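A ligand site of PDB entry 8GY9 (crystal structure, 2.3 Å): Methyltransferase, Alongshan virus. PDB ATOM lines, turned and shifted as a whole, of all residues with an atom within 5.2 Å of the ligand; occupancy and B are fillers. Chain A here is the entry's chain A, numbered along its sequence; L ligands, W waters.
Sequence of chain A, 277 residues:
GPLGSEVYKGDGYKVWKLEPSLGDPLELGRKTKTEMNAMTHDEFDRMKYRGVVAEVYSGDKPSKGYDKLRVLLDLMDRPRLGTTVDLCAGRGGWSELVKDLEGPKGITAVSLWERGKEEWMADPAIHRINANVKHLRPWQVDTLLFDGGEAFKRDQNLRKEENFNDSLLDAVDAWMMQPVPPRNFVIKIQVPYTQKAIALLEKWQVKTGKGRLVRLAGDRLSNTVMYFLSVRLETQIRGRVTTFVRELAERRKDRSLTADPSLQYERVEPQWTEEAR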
ATOM      1  N   SER A  63     -15.967   9.345  -1.329  1.00  0.00           N
ATOM      2  CA  SER A  63     -15.971   9.111   0.113  1.00  0.00           C
ATOM      3  C   SER A  63     -14.522   9.107   0.576  1.00  0.00           C
ATOM      4  O   SER A  63     -13.587   9.297  -0.211  1.00  0.00           O
ATOM      5  CB  SER A  63     -16.676   7.801   0.465  1.00  0.00           C
ATOM      6  OG  SER A  63     -15.838   6.681   0.213  1.00  0.00           O
ATOM      7  N   GLY A  65     -13.252   6.407   1.668  1.00  0.00           N
ATOM      8  CA  GLY A  65     -12.770   5.074   1.347  1.00  0.00           C
ATOM      9  C   GLY A  65     -11.767   5.068   0.213  1.00  0.00           C
ATOM     10  O   GLY A  65     -10.894   4.192   0.153  1.00  0.00           O
ATOM     11  N   TYR A  66     -11.863   6.054  -0.686  1.00  0.00           N
ATOM     12  CA  TYR A  66     -10.948   6.174  -1.827  1.00  0.00           C
ATOM     13  C   TYR A  66      -9.481   6.175  -1.373  1.00  0.00           C
ATOM     14  O   TYR A  66      -8.668   5.372  -1.848  1.00  0.00           O
ATOM     15  CB  TYR A  66     -11.268   7.463  -2.578  1.00  0.00           C
ATOM     16  CG  TYR A  66     -10.536   7.642  -3.881  1.00  0.00           C
ATOM     17  CD1 TYR A  66      -9.228   8.102  -3.919  1.00  0.00           C
ATOM     18  CD2 TYR A  66     -11.171   7.378  -5.092  1.00  0.00           C
ATOM     19  CE1 TYR A  66      -8.573   8.274  -5.126  1.00  0.00           C
ATOM     20  CE2 TYR A  66     -10.543   7.540  -6.269  1.00  0.00           C
ATOM     21  CZ  TYR A  66      -9.249   7.981  -6.300  1.00  0.00           C
ATOM     22  OH  TYR A  66      -8.644   8.129  -7.529  1.00  0.00           O
ATOM     23  N   ASP A  86     -16.556  -5.369  -5.894  1.00  0.00           N
ATOM     24  CA  ASP A  86     -16.560  -4.529  -4.704  1.00  0.00           C
ATOM     25  C   ASP A  86     -17.831  -4.868  -3.910  1.00  0.00           C
ATOM     26  O   ASP A  86     -18.922  -4.408  -4.246  1.00  0.00           O
ATOM     27  CB  ASP A  86     -16.521  -3.061  -5.126  1.00  0.00           C
ATOM     28  CG  ASP A  86     -16.321  -2.094  -3.962  1.00  0.00           C
ATOM     29  OD1 ASP A  86     -16.053  -2.544  -2.820  1.00  0.00           O
ATOM     30  OD2 ASP A  86     -16.399  -0.865  -4.209  1.00  0.00           O
ATOM     31  N   CYS A  88     -20.272  -4.678  -0.686  1.00  0.00           N
ATOM     32  CA  CYS A  88     -20.657  -3.569   0.192  1.00  0.00           C
ATOM     33  C   CYS A  88     -20.032  -2.260  -0.270  1.00  0.00           C
ATOM     34  O   CYS A  88     -19.308  -1.595   0.467  1.00  0.00           O
ATOM     35  CB  CYS A  88     -20.300  -3.854   1.650  1.00  0.00           C
ATOM     36  SG  CYS A  88     -20.981  -5.376   2.264  1.00  0.00           S
ATOM     37  N   ALA A  89     -20.304  -1.903  -1.519  1.00  0.00           N
ATOM     38  CA  ALA A  89     -19.630  -0.765  -2.122  1.00  0.00           C
ATOM     39  C   ALA A  89     -20.122   0.578  -1.567  1.00  0.00           C
ATOM     40  O   ALA A  89     -19.376   1.557  -1.600  1.00  0.00           O
ATOM     41  CB  ALA A  89     -19.803  -0.795  -3.635  1.00  0.00           C
ATOM     42  N   GLY A  90     -21.369   0.642  -1.079  1.00  0.00           N
ATOM     43  CA  GLY A  90     -21.894   1.865  -0.497  1.00  0.00           C
ATOM     44  C   GLY A  90     -21.909   3.007  -1.511  1.00  0.00           C
ATOM     45  O   GLY A  90     -22.469   2.902  -2.597  1.00  0.00           O
ATOM     46  N   ARG A  91     -21.260   4.119  -1.157  1.00  0.00           N
ATOM     47  CA  ARG A  91     -21.190   5.263  -2.048  1.00  0.00           C
ATOM     48  C   ARG A  91     -20.213   5.071  -3.206  1.00  0.00           C
ATOM     49  O   ARG A  91     -20.248   5.850  -4.155  1.00  0.00           O
ATOM     50  CB  ARG A  91     -20.826   6.515  -1.259  1.00  0.00           C
ATOM     51  CG  ARG A  91     -21.691   6.700  -0.047  1.00  0.00           C
ATOM     52  CD  ARG A  91     -21.621   8.127   0.475  1.00  0.00           C
ATOM     53  NE  ARG A  91     -20.973   8.218   1.770  1.00  0.00           N
ATOM     54  CZ  ARG A  91     -20.368   9.326   2.194  1.00  0.00           C
ATOM     55  NH1 ARG A  91     -20.344  10.402   1.423  1.00  0.00           N
ATOM     56  NH2 ARG A  91     -19.781   9.354   3.378  1.00  0.00           N
ATOM     57  N   GLY A  92     -19.335   4.078  -3.123  1.00  0.00           N
ATOM     58  CA  GLY A  92     -18.481   3.735  -4.246  1.00  0.00           C
ATOM     59  C   GLY A  92     -17.076   4.304  -4.257  1.00  0.00           C
ATOM     60  O   GLY A  92     -16.461   4.335  -5.330  1.00  0.00           O
ATOM     61  N   GLY A  93     -16.523   4.716  -3.118  1.00  0.00           N
ATOM     62  CA  GLY A  93     -15.158   5.224  -3.130  1.00  0.00           C
ATOM     63  C   GLY A  93     -14.148   4.203  -3.645  1.00  0.00           C
ATOM     64  O   GLY A  93     -13.298   4.516  -4.479  1.00  0.00           O
ATOM     65  N   TRP A  94     -14.249   2.963  -3.165  1.00  0.00           N
ATOM     66  CA  TRP A  94     -13.351   1.908  -3.622  1.00  0.00           C
ATOM     67  C   TRP A  94     -13.516   1.644  -5.119  1.00  0.00           C
ATOM     68  O   TRP A  94     -12.526   1.632  -5.874  1.00  0.00           O
ATOM     69  CB  TRP A  94     -13.598   0.620  -2.820  1.00  0.00           C
ATOM     70  CG  TRP A  94     -13.063   0.686  -1.420  1.00  0.00           C
ATOM     71  CD1 TRP A  94     -12.730   1.808  -0.724  1.00  0.00           C
ATOM     72  CD2 TRP A  94     -12.781  -0.427  -0.549  1.00  0.00           C
ATOM     73  NE1 TRP A  94     -12.259   1.472   0.519  1.00  0.00           N
ATOM     74  CE2 TRP A  94     -12.292   0.110   0.651  1.00  0.00           C
ATOM     75  CE3 TRP A  94     -12.896  -1.818  -0.685  1.00  0.00           C
ATOM     76  CZ2 TRP A  94     -11.910  -0.691   1.718  1.00  0.00           C
ATOM     77  CZ3 TRP A  94     -12.526  -2.608   0.388  1.00  0.00           C
ATOM     78  CH2 TRP A  94     -12.042  -2.042   1.575  1.00  0.00           C
ATOM     79  N   VAL A 110     -21.455  -4.210  -5.551  1.00  0.00           N
ATOM     80  CA  VAL A 110     -22.589  -4.846  -4.892  1.00  0.00           C
ATOM     81  C   VAL A 110     -22.841  -4.147  -3.566  1.00  0.00           C
ATOM     82  O   VAL A 110     -21.915  -3.995  -2.761  1.00  0.00           O
ATOM     83  CB  VAL A 110     -22.344  -6.345  -4.685  1.00  0.00           C
ATOM     84  CG1 VAL A 110     -23.524  -6.964  -3.947  1.00  0.00           C
ATOM     85  CG2 VAL A 110     -22.092  -7.043  -6.011  1.00  0.00           C
ATOM     86  N   SER A 111     -24.079  -3.716  -3.343  1.00  0.00           N
ATOM     87  CA  SER A 111     -24.436  -3.025  -2.114  1.00  0.00           C
ATOM     88  C   SER A 111     -25.951  -3.031  -1.940  1.00  0.00           C
ATOM     89  O   SER A 111     -26.695  -3.443  -2.839  1.00  0.00           O
ATOM     90  CB  SER A 111     -23.894  -1.587  -2.117  1.00  0.00           C
ATOM     91  OG  SER A 111     -23.664  -1.113  -0.800  1.00  0.00           O
ATOM     92  N   LEU A 112     -26.429  -2.550  -0.820  1.00  0.00           N
ATOM     93  CA  LEU A 112     -27.836  -2.425  -0.585  1.00  0.00           C
ATOM     94  C   LEU A 112     -28.122  -0.934  -0.605  1.00  0.00           C
ATOM     95  O   LEU A 112     -27.768  -0.240   0.311  1.00  0.00           O
ATOM     96  CB  LEU A 112     -28.234  -3.008   0.746  1.00  0.00           C
ATOM     97  CG  LEU A 112     -28.686  -4.455   0.624  1.00  0.00           C
ATOM     98  CD1 LEU A 112     -28.709  -5.199   1.935  1.00  0.00           C
ATOM     99  CD2 LEU A 112     -30.020  -4.518  -0.039  1.00  0.00           C
ATOM    100  N   GLU A 118     -27.571   5.309   1.692  1.00  0.00           N
ATOM    101  CA  GLU A 118     -26.444   5.481   0.769  1.00  0.00           C
ATOM    102  C   GLU A 118     -26.946   5.689  -0.654  1.00  0.00           C
ATOM    103  O   GLU A 118     -27.765   4.924  -1.159  1.00  0.00           O
ATOM    104  CB  GLU A 118     -25.494   4.271   0.796  1.00  0.00           C
ATOM    105  CG  GLU A 118     -25.365   3.569   2.132  1.00  0.00           C
ATOM    106  CD  GLU A 118     -24.530   4.336   3.144  1.00  0.00           C
ATOM    107  OE1 GLU A 118     -23.728   5.199   2.744  1.00  0.00           O
ATOM    108  OE2 GLU A 118     -24.658   4.044   4.357  1.00  0.00           O
ATOM    109  N   ALA A 131     -28.069  -5.618  -4.121  1.00  0.00           N
ATOM    110  CA  ALA A 131     -28.330  -6.905  -3.503  1.00  0.00           C
ATOM    111  C   ALA A 131     -27.626  -7.033  -2.160  1.00  0.00           C
ATOM    112  O   ALA A 131     -26.676  -6.310  -1.856  1.00  0.00           O
ATOM    113  CB  ALA A 131     -27.860  -8.056  -4.399  1.00  0.00           C
ATOM    114  N   ASN A 132     -28.100  -7.996  -1.361  1.00  0.00           N
ATOM    115  CA  ASN A 132     -27.483  -8.357  -0.097  1.00  0.00           C
ATOM    116  C   ASN A 132     -26.329  -9.324  -0.368  1.00  0.00           C
ATOM    117  O   ASN A 132     -26.548 -10.431  -0.877  1.00  0.00           O
ATOM    118  CB  ASN A 132     -28.527  -8.985   0.834  1.00  0.00           C
ATOM    119  CG  ASN A 132     -28.005  -9.275   2.248  1.00  0.00           C
ATOM    120  OD1 ASN A 132     -26.816  -9.524   2.467  1.00  0.00           O
ATOM    121  ND2 ASN A 132     -28.927  -9.253   3.207  1.00  0.00           N
ATOM    122  N   VAL A 133     -25.106  -8.929   0.003  1.00  0.00           N
ATOM    123  CA  VAL A 133     -23.940  -9.753  -0.342  1.00  0.00           C
ATOM    124  C   VAL A 133     -24.070 -11.157   0.236  1.00  0.00           C
ATOM    125  O   VAL A 133     -23.497 -12.108  -0.296  1.00  0.00           O
ATOM    126  CB  VAL A 133     -22.630  -9.079   0.091  1.00  0.00           C
ATOM    127  CG1 VAL A 133     -22.545  -7.672  -0.480  1.00  0.00           C
ATOM    128  CG2 VAL A 133     -22.489  -9.056   1.605  1.00  0.00           C
ATOM    129  N   LYS A 134     -24.832 -11.322   1.331  1.00  0.00           N
ATOM    130  CA  LYS A 134     -25.078 -12.661   1.856  1.00  0.00           C
ATOM    131  C   LYS A 134     -25.887 -13.500   0.896  1.00  0.00           C
ATOM    132  O   LYS A 134     -25.855 -14.731   0.983  1.00  0.00           O
ATOM    133  CB  LYS A 134     -25.811 -12.611   3.202  1.00  0.00           C
ATOM    134  CG  LYS A 134     -24.999 -12.076   4.349  1.00  0.00           C
ATOM    135  CD  LYS A 134     -25.723 -12.350   5.658  1.00  0.00           C
ATOM    136  CE  LYS A 134     -25.416 -11.290   6.677  1.00  0.00           C
ATOM    137  NZ  LYS A 134     -26.132 -11.521   7.957  1.00  0.00           N
ATOM    138  N   ASP A 147     -15.775  -4.275   1.966  1.00  0.00           N
ATOM    139  CA  ASP A 147     -15.763  -3.180   2.929  1.00  0.00           C
ATOM    140  C   ASP A 147     -16.992  -3.205   3.830  1.00  0.00           C
ATOM    141  O   ASP A 147     -17.394  -2.176   4.377  1.00  0.00           O
ATOM    142  CB  ASP A 147     -15.638  -1.829   2.220  1.00  0.00           C
ATOM    143  CG  ASP A 147     -15.051  -0.739   3.121  1.00  0.00           C
ATOM    144  OD1 ASP A 147     -14.461  -1.055   4.176  1.00  0.00           O
ATOM    145  OD2 ASP A 147     -15.152   0.455   2.743  1.00  0.00           O
ATOM    146  N   GLY A 148     -17.619  -4.366   3.989  1.00  0.00           N
ATOM    147  CA  GLY A 148     -18.739  -4.469   4.899  1.00  0.00           C
ATOM    148  C   GLY A 148     -18.268  -4.453   6.349  1.00  0.00           C
ATOM    149  O   GLY A 148     -17.082  -4.536   6.661  1.00  0.00           O
ATOM    150  N   GLY A 149     -19.238  -4.334   7.250  1.00  0.00           N
ATOM    151  CA  GLY A 149     -18.924  -4.237   8.667  1.00  0.00           C
ATOM    152  C   GLY A 149     -19.655  -3.089   9.324  1.00  0.00           C
ATOM    153  O   GLY A 149     -19.727  -2.000   8.759  1.00  0.00           O
ATOM    154  N   GLU A 150     -20.195  -3.326  10.514  1.00  0.00           N
ATOM    155  CA  GLU A 150     -20.971  -2.328  11.244  1.00  0.00           C
ATOM    156  C   GLU A 150     -20.575  -2.311  12.708  1.00  0.00           C
ATOM    157  O   GLU A 150     -20.478  -3.371  13.338  1.00  0.00           O
ATOM    158  CB  GLU A 150     -22.484  -2.603  11.128  1.00  0.00           C
ATOM    159  CG  GLU A 150     -23.073  -2.455   9.727  1.00  0.00           C
ATOM    160  CD  GLU A 150     -23.150  -1.013   9.269  1.00  0.00           C
ATOM    161  OE1 GLU A 150     -22.946  -0.122  10.122  1.00  0.00           O
ATOM    162  OE2 GLU A 150     -23.416  -0.770   8.075  1.00  0.00           O
ATOM    163  N   PHE A 164     -23.096 -10.375  14.300  1.00  0.00           N
ATOM    164  CA  PHE A 164     -23.479  -9.723  13.053  1.00  0.00           C
ATOM    165  C   PHE A 164     -22.299  -9.631  12.097  1.00  0.00           C
ATOM    166  O   PHE A 164     -22.406  -9.963  10.897  1.00  0.00           O
ATOM    167  CB  PHE A 164     -24.025  -8.333  13.373  1.00  0.00           C
ATOM    168  CG  PHE A 164     -24.354  -7.495  12.159  1.00  0.00           C
ATOM    169  CD1 PHE A 164     -23.376  -6.700  11.561  1.00  0.00           C
ATOM    170  CD2 PHE A 164     -25.640  -7.488  11.630  1.00  0.00           C
ATOM    171  CE1 PHE A 164     -23.665  -5.927  10.431  1.00  0.00           C
ATOM    172  CE2 PHE A 164     -25.938  -6.718  10.504  1.00  0.00           C
ATOM    173  CZ  PHE A 164     -24.957  -5.936   9.904  1.00  0.00           C
ATOM    174  N   LEU A 168     -21.376 -11.550   8.433  1.00  0.00           N
ATOM    175  CA  LEU A 168     -20.907 -10.957   7.177  1.00  0.00           C
ATOM    176  C   LEU A 168     -19.632 -11.648   6.647  1.00  0.00           C
ATOM    177  O   LEU A 168     -19.536 -11.989   5.456  1.00  0.00           O
ATOM    178  CB  LEU A 168     -20.655  -9.465   7.367  1.00  0.00           C
ATOM    179  CG  LEU A 168     -21.818  -8.527   7.058  1.00  0.00           C
ATOM    180  CD1 LEU A 168     -21.463  -7.127   7.531  1.00  0.00           C
ATOM    181  CD2 LEU A 168     -22.065  -8.525   5.557  1.00  0.00           C
ATOM    182  N   LYS A 188     -12.081  -5.980   4.671  1.00  0.00           N
ATOM    183  CA  LYS A 188     -12.223  -5.301   5.951  1.00  0.00           C
ATOM    184  C   LYS A 188     -12.680  -6.279   7.003  1.00  0.00           C
ATOM    185  O   LYS A 188     -13.575  -7.092   6.775  1.00  0.00           O
ATOM    186  CB  LYS A 188     -13.228  -4.148   5.850  1.00  0.00           C
ATOM    187  CG  LYS A 188     -13.501  -3.509   7.212  1.00  0.00           C
ATOM    188  CD  LYS A 188     -13.974  -2.071   7.114  1.00  0.00           C
ATOM    189  CE  LYS A 188     -15.371  -1.925   7.652  1.00  0.00           C
ATOM    190  NZ  LYS A 188     -16.042  -0.740   7.064  1.00  0.00           N
HETATM  191  N1  LIG L   1     -16.099   1.066   0.349  1.00  0.00           N
HETATM  192  C1  LIG L   1     -17.090   2.139   0.409  1.00  0.00           C
HETATM  193  C2  LIG L   1     -16.555   3.498  -0.040  1.00  0.00           C
HETATM  194  O1  LIG L   1     -17.325   4.458  -0.114  1.00  0.00           O
HETATM  195  O2  LIG L   1     -15.367   3.662  -0.328  1.00  0.00           O
HETATM  196  C3  LIG L   1     -17.701   2.288   1.802  1.00  0.00           C
HETATM  197  C4  LIG L   1     -18.208   0.997   2.434  1.00  0.00           C
HETATM  198  S1  LIG L   1     -19.668   1.319   3.453  1.00  0.00           S
HETATM  199  C5  LIG L   1     -18.919   1.545   5.091  1.00  0.00           C
HETATM  200  C6  LIG L   1     -20.416  -0.317   3.596  1.00  0.00           C
HETATM  201  C7  LIG L   1     -21.746  -0.386   2.868  1.00  0.00           C
HETATM  202  O3  LIG L   1     -22.218  -1.712   2.801  1.00  0.00           O
HETATM  203  C8  LIG L   1     -22.830   0.421   3.567  1.00  0.00           C
HETATM  204  O4  LIG L   1     -23.162   1.503   2.738  1.00  0.00           O
HETATM  205  C9  LIG L   1     -24.023  -0.517   3.683  1.00  0.00           C
HETATM  206  O5  LIG L   1     -25.154   0.085   3.103  1.00  0.00           O
HETATM  207  C10 LIG L   1     -23.631  -1.748   2.883  1.00  0.00           C
HETATM  208  N2  LIG L   1     -24.057  -3.023   3.482  1.00  0.00           N
HETATM  209  C11 LIG L   1     -24.158  -3.363   4.809  1.00  0.00           C
HETATM  210  N3  LIG L   1     -24.582  -4.657   4.899  1.00  0.00           N
HETATM  211  C12 LIG L   1     -24.736  -5.133   3.639  1.00  0.00           C
HETATM  212  C13 LIG L   1     -25.125  -6.363   3.132  1.00  0.00           C
HETATM  213  N4  LIG L   1     -25.462  -7.381   3.941  1.00  0.00           N
HETATM  214  N5  LIG L   1     -25.178  -6.540   1.767  1.00  0.00           N
HETATM  215  C14 LIG L   1     -24.859  -5.520   0.902  1.00  0.00           C
HETATM  216  N6  LIG L   1     -24.466  -4.304   1.408  1.00  0.00           N
HETATM  217  C15 LIG L   1     -24.407  -4.116   2.746  1.00  0.00           C
HETATM  218  O   HOH W   1     -16.818   1.180  -2.984  1.00  0.00           O
HETATM  219  O   HOH W   2     -16.540  -1.172  -0.786  1.00  0.00           O
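The side-chain carboxylate of Asp 147 is in salt-bridge range of a nitrogen (N1) of the ligand (2.6 Å).
OG of Ser 63 is in hydrogen-bond range of O1 of the ligand.
The side-chain amide oxygen of Asn 132 lies within hydrogen-bond range of a nitrogen (N4) of the ligand (2.9 Å).
The backbone NH (N) of Val 133 sits at hydrogen-bond distance from a nitrogen (N5) of the ligand.
The side-chain carboxylate (OE2) of Glu 118 lies close to an oxygen (O4) of the ligand (3.4 Å).
A nitrogen (N6) of the ligand sits close to the side-chain sulfur (SG) of Cys 88 (3.7 Å).
An oxygen (O1) of the ligand sits at hydrogen-bond distance from the backbone NH (N) of Gly 93 (3.1 Å).
An oxygen (O2) of the ligand lies within hydrogen-bond range of the backbone NH (N) of Trp 94 (3.1 Å).
The backbone NH of Leu 112 lies within hydrogen-bond range of a nitrogen (N6) of the ligand, 3.4 Å away.
OD1 of Asp 147 is in salt-bridge range of NZ of Lys 188, at 3.3 Å.
The side-chain hydroxyl (OG) of Ser 63 lies within hydrogen-bond range of the backbone NH (N) of Gly 65.
The side-chain amide oxygen of Asn 132 is in hydrogen-bond range of the backbone NH of Lys 134, 2.9 Å away.
The backbone NH (N) of Cys 88 lies within hydrogen-bond range of the backbone carbonyl oxygen (O) of Val 110, 2.7 Å away.
The backbone carbonyl oxygen (O) of Val 110 lies within hydrogen-bond range of the backbone NH (N) of Ala 89.
The indole nitrogen of Trp 94 is in hydrogen-bond range of the backbone carbonyl oxygen of Gly 65.
The backbone NH (N) of Ala 131 lies within hydrogen-bond range of the backbone carbonyl oxygen (O) of Ser 111 (2.9 Å).
N of Gly 90 is in hydrogen-bond range of OG of Ser 111, 2.9 Å away.
Merely in contact with the ligand: Gly 65, Ala 89, Gly 90, Gly 92, Ser 111, Ala 131 and Leu 168.
The nearest printed residue that does not touch the ligand is Arg 91 (4.1 Å).
Water W2 lies within hydrogen-bond range of the side-chain carboxylate (OD1) of Asp 86 (2.5 Å), a nitrogen (N1) of the ligand (2.5 Å) and the backbone carbonyl oxygen (O) of Cys 88 (3.1 Å).
Water W1 lies within hydrogen-bond range of OD2 of Asp 86, O of Ala 89, N of Trp 94 and N1 of the ligand.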
